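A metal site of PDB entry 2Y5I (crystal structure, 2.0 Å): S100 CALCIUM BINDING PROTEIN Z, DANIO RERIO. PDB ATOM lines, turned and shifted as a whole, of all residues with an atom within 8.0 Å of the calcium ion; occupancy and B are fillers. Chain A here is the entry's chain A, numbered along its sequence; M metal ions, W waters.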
ATOM      1  N   LYS A  28      19.385  32.103   4.851  1.00  0.00           N
ATOM      2  CA  LYS A  28      18.553  30.941   4.541  1.00  0.00           C
ATOM      3  C   LYS A  28      18.353  30.821   3.041  1.00  0.00           C
ATOM      4  O   LYS A  28      18.318  31.825   2.296  1.00  0.00           O
ATOM      5  CB  LYS A  28      17.202  31.036   5.229  1.00  0.00           C
ATOM      6  CG  LYS A  28      17.230  31.227   6.742  1.00  0.00           C
ATOM      7  CD  LYS A  28      15.813  31.256   7.259  1.00  0.00           C
ATOM      8  CE  LYS A  28      15.677  31.585   8.723  1.00  0.00           C
ATOM      9  NZ  LYS A  28      14.200  31.906   9.022  1.00  0.00           N
ATOM     10  N   LEU A  29      18.135  29.579   2.611  1.00  0.00           N
ATOM     11  CA  LEU A  29      17.839  29.310   1.225  1.00  0.00           C
ATOM     12  C   LEU A  29      16.337  29.305   0.938  1.00  0.00           C
ATOM     13  O   LEU A  29      15.575  28.528   1.528  1.00  0.00           O
ATOM     14  CB  LEU A  29      18.435  27.971   0.809  1.00  0.00           C
ATOM     15  CG  LEU A  29      19.939  27.760   0.908  1.00  0.00           C
ATOM     16  CD1 LEU A  29      20.241  26.257   0.925  1.00  0.00           C
ATOM     17  CD2 LEU A  29      20.643  28.446  -0.269  1.00  0.00           C
ATOM     18  N   MET A  59      12.841  20.381  -0.877  1.00  0.00           N
ATOM     19  CA  MET A  59      12.402  21.573  -0.115  1.00  0.00           C
ATOM     20  C   MET A  59      11.486  21.201   1.068  1.00  0.00           C
ATOM     21  O   MET A  59      11.786  21.538   2.216  1.00  0.00           O
ATOM     22  CB  MET A  59      11.666  22.565  -1.037  1.00  0.00           C
ATOM     23  CG  MET A  59      11.321  23.899  -0.411  1.00  0.00           C
ATOM     24  SD  MET A  59      12.810  24.851  -0.038  1.00  0.00           S
ATOM     25  CE  MET A  59      12.007  26.144   0.945  1.00  0.00           C
ATOM     26  N   LEU A  62      13.387  19.087   3.750  1.00  0.00           N
ATOM     27  CA  LEU A  62      14.426  19.845   4.471  1.00  0.00           C
ATOM     28  C   LEU A  62      13.860  20.954   5.352  1.00  0.00           C
ATOM     29  O   LEU A  62      14.453  21.249   6.367  1.00  0.00           O
ATOM     30  CB  LEU A  62      15.459  20.435   3.511  1.00  0.00           C
ATOM     31  CG  LEU A  62      16.292  19.422   2.735  1.00  0.00           C
ATOM     32  CD1 LEU A  62      17.295  20.147   1.888  1.00  0.00           C
ATOM     33  CD2 LEU A  62      17.012  18.357   3.689  1.00  0.00           C
ATOM     34  N   ASP A  63      12.767  21.583   4.943  1.00  0.00           N
ATOM     35  CA  ASP A  63      12.181  22.668   5.735  1.00  0.00           C
ATOM     36  C   ASP A  63      11.359  22.108   6.903  1.00  0.00           C
ATOM     37  O   ASP A  63      10.131  22.171   6.892  1.00  0.00           O
ATOM     38  CB  ASP A  63      11.297  23.553   4.843  1.00  0.00           C
ATOM     39  CG  ASP A  63      10.704  24.715   5.610  1.00  0.00           C
ATOM     40  OD1 ASP A  63      11.255  25.121   6.656  1.00  0.00           O
ATOM     41  OD2 ASP A  63       9.654  25.154   5.201  1.00  0.00           O
ATOM     42  N   SER A  64      12.057  21.590   7.912  1.00  0.00           N
ATOM     43  CA  SER A  64      11.397  20.967   9.074  1.00  0.00           C
ATOM     44  C   SER A  64      10.541  21.878   9.909  1.00  0.00           C
ATOM     45  O   SER A  64       9.584  21.427  10.516  1.00  0.00           O
ATOM     46  CB  SER A  64      12.395  20.431  10.076  1.00  0.00           C
ATOM     47  OG  SER A  64      13.393  19.713   9.505  1.00  0.00           O
ATOM     48  N   ASN A  65      10.912  23.166   9.994  1.00  0.00           N
ATOM     49  CA  ASN A  65      10.137  24.074  10.815  1.00  0.00           C
ATOM     50  C   ASN A  65       9.119  24.867   9.994  1.00  0.00           C
ATOM     51  O   ASN A  65       8.416  25.731  10.525  1.00  0.00           O
ATOM     52  CB  ASN A  65      11.049  24.989  11.613  1.00  0.00           C
ATOM     53  CG  ASN A  65      11.836  25.932  10.739  1.00  0.00           C
ATOM     54  OD1 ASN A  65      11.861  25.816   9.523  1.00  0.00           O
ATOM     55  ND2 ASN A  65      12.438  26.915  11.366  1.00  0.00           N
ATOM     56  N   LYS A  66       9.048  24.596   8.698  1.00  0.00           N
ATOM     57  CA  LYS A  66       7.950  25.118   7.901  1.00  0.00           C
ATOM     58  C   LYS A  66       7.937  26.639   7.812  1.00  0.00           C
ATOM     59  O   LYS A  66       6.903  27.231   7.826  1.00  0.00           O
ATOM     60  CB  LYS A  66       6.617  24.581   8.452  1.00  0.00           C
ATOM     61  CG  LYS A  66       6.283  23.225   7.796  1.00  0.00           C
ATOM     62  CD  LYS A  66       6.131  22.083   8.764  1.00  0.00           C
ATOM     63  CE  LYS A  66       6.041  20.756   7.996  1.00  0.00           C
ATOM     64  NZ  LYS A  66       5.176  19.775   8.750  1.00  0.00           N
ATOM     65  N   ASP A  67       9.117  27.259   7.721  1.00  0.00           N
ATOM     66  CA  ASP A  67       9.205  28.725   7.496  1.00  0.00           C
ATOM     67  C   ASP A  67       9.422  29.091   6.021  1.00  0.00           C
ATOM     68  O   ASP A  67       9.696  30.232   5.683  1.00  0.00           O
ATOM     69  CB  ASP A  67      10.244  29.361   8.384  1.00  0.00           C
ATOM     70  CG  ASP A  67      11.641  28.873   8.159  1.00  0.00           C
ATOM     71  OD1 ASP A  67      11.919  28.042   7.250  1.00  0.00           O
ATOM     72  OD2 ASP A  67      12.473  29.360   8.941  1.00  0.00           O
ATOM     73  N   ASN A  68       9.261  28.097   5.161  1.00  0.00           N
ATOM     74  CA  ASN A  68       9.473  28.202   3.729  1.00  0.00           C
ATOM     75  C   ASN A  68      10.936  28.514   3.348  1.00  0.00           C
ATOM     76  O   ASN A  68      11.202  29.023   2.231  1.00  0.00           O
ATOM     77  CB  ASN A  68       8.541  29.231   3.117  1.00  0.00           C
ATOM     78  CG  ASN A  68       8.196  28.916   1.713  1.00  0.00           C
ATOM     79  OD1 ASN A  68       8.077  27.756   1.366  1.00  0.00           O
ATOM     80  ND2 ASN A  68       8.051  29.905   0.900  1.00  0.00           N
ATOM     81  N   GLU A  69      11.876  28.192   4.237  1.00  0.00           N
ATOM     82  CA  GLU A  69      13.314  28.358   3.926  1.00  0.00           C
ATOM     83  C   GLU A  69      14.054  27.148   4.404  1.00  0.00           C
ATOM     84  O   GLU A  69      13.574  26.415   5.286  1.00  0.00           O
ATOM     85  CB  GLU A  69      13.912  29.527   4.688  1.00  0.00           C
ATOM     86  CG  GLU A  69      13.131  30.774   4.641  1.00  0.00           C
ATOM     87  CD  GLU A  69      13.378  31.577   3.414  1.00  0.00           C
ATOM     88  OE1 GLU A  69      14.496  31.541   2.876  1.00  0.00           O
ATOM     89  OE2 GLU A  69      12.455  32.292   2.994  1.00  0.00           O
ATOM     90  N   VAL A  70      15.248  26.963   3.844  1.00  0.00           N
ATOM     91  CA  VAL A  70      16.177  25.957   4.307  1.00  0.00           C
ATOM     92  C   VAL A  70      17.334  26.721   4.962  1.00  0.00           C
ATOM     93  O   VAL A  70      18.202  27.308   4.284  1.00  0.00           O
ATOM     94  CB  VAL A  70      16.679  25.078   3.154  1.00  0.00           C
ATOM     95  CG1 VAL A  70      17.843  24.172   3.596  1.00  0.00           C
ATOM     96  CG2 VAL A  70      15.521  24.218   2.555  1.00  0.00           C
ATOM     97  N   ASP A  71      17.324  26.758   6.299  1.00  0.00           N
ATOM     98  CA  ASP A  71      18.432  27.394   7.019  1.00  0.00           C
ATOM     99  C   ASP A  71      19.685  26.523   7.024  1.00  0.00           C
ATOM    100  O   ASP A  71      19.738  25.394   6.455  1.00  0.00           O
ATOM    101  CB  ASP A  71      18.000  27.840   8.421  1.00  0.00           C
ATOM    102  CG  ASP A  71      17.674  26.697   9.347  1.00  0.00           C
ATOM    103  OD1 ASP A  71      18.183  25.570   9.211  1.00  0.00           O
ATOM    104  OD2 ASP A  71      16.811  26.919  10.225  1.00  0.00           O
ATOM    105  N   PHE A  72      20.743  27.018   7.680  1.00  0.00           N
ATOM    106  CA  PHE A  72      22.009  26.258   7.583  1.00  0.00           C
ATOM    107  C   PHE A  72      21.955  24.888   8.261  1.00  0.00           C
ATOM    108  O   PHE A  72      22.475  23.911   7.761  1.00  0.00           O
ATOM    109  CB  PHE A  72      23.181  27.069   8.090  1.00  0.00           C
ATOM    110  CG  PHE A  72      24.520  26.411   7.792  1.00  0.00           C
ATOM    111  CD1 PHE A  72      24.995  26.354   6.495  1.00  0.00           C
ATOM    112  CD2 PHE A  72      25.274  25.812   8.788  1.00  0.00           C
ATOM    113  CE1 PHE A  72      26.234  25.766   6.218  1.00  0.00           C
ATOM    114  CE2 PHE A  72      26.512  25.233   8.514  1.00  0.00           C
ATOM    115  CZ  PHE A  72      26.975  25.190   7.240  1.00  0.00           C
ATOM    116  N   GLU A  74      19.331  23.103   8.561  1.00  0.00           N
ATOM    117  CA  GLU A  74      18.564  22.275   7.684  1.00  0.00           C
ATOM    118  C   GLU A  74      19.350  21.797   6.460  1.00  0.00           C
ATOM    119  O   GLU A  74      19.127  20.652   6.017  1.00  0.00           O
ATOM    120  CB  GLU A  74      17.280  22.958   7.253  1.00  0.00           C
ATOM    121  CG  GLU A  74      16.248  23.052   8.365  1.00  0.00           C
ATOM    122  CD  GLU A  74      15.106  24.066   8.057  1.00  0.00           C
ATOM    123  OE1 GLU A  74      15.313  25.040   7.272  1.00  0.00           O
ATOM    124  OE2 GLU A  74      14.029  23.920   8.648  1.00  0.00           O
ATOM    125  N   PHE A  75      20.208  22.664   5.919  1.00  0.00           N
ATOM    126  CA  PHE A  75      21.086  22.348   4.790  1.00  0.00           C
ATOM    127  C   PHE A  75      22.065  21.247   5.206  1.00  0.00           C
ATOM    128  O   PHE A  75      22.309  20.317   4.429  1.00  0.00           O
ATOM    129  CB  PHE A  75      21.821  23.580   4.329  1.00  0.00           C
ATOM    130  CG  PHE A  75      22.923  23.324   3.337  1.00  0.00           C
ATOM    131  CD1 PHE A  75      22.649  22.847   2.053  1.00  0.00           C
ATOM    132  CD2 PHE A  75      24.238  23.564   3.677  1.00  0.00           C
ATOM    133  CE1 PHE A  75      23.674  22.642   1.139  1.00  0.00           C
ATOM    134  CE2 PHE A  75      25.248  23.354   2.775  1.00  0.00           C
ATOM    135  CZ  PHE A  75      24.977  22.896   1.504  1.00  0.00           C
HETATM  136 CA    CA M   1      13.171  25.975   7.551  1.00  0.00          CA
HETATM  137  O   HOH W   1      14.630  27.602   8.534  1.00  0.00           O
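Of the 16 residues printed, 5 come within 4 Å of the calcium ion. Along chain A the residues within 4 Å of the calcium ion span positions 63 to 74. The nearest printed residue that does not touch the calcium ion is Val 70 (4.4 Å).
Water W1 lies within hydrogen-bond range of the side-chain carboxylate of Asp 67 and the side-chain carboxylate of Asp 71.
The calcium ion is bound by OD1 of Asp 63 (2.3 Å). O of Glu 69 binds the calcium ion. OE1 of Glu 74 is bound to the calcium ion, at 2.4 Å. The side-chain amide oxygen (OD1) of Asn 65 binds the calcium ion (2.4 Å). Water W1 binds the calcium ion (2.4 Å). OD1 of Asp 67 is bound to the calcium ion, 2.4 Å away. The side-chain carboxylate (OE2) of Glu 74 binds the calcium ion (2.5 Å).
N of Lys 66 lies close to OD1 of Asp 63, at 3.1 Å. N of Asn 68 lies within hydrogen-bond range of OD2 of Asp 63 (3.0 Å). The side-chain carboxylate (OD1) of Asp 71 is in hydrogen-bond range of the backbone NH (N) of Glu 74. OE2 of Glu 74 sits close to N of Ser 64 (3.1 Å). NZ of Lys 28 is in salt-bridge range of OD2 of Asp 67 (3.1 Å).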
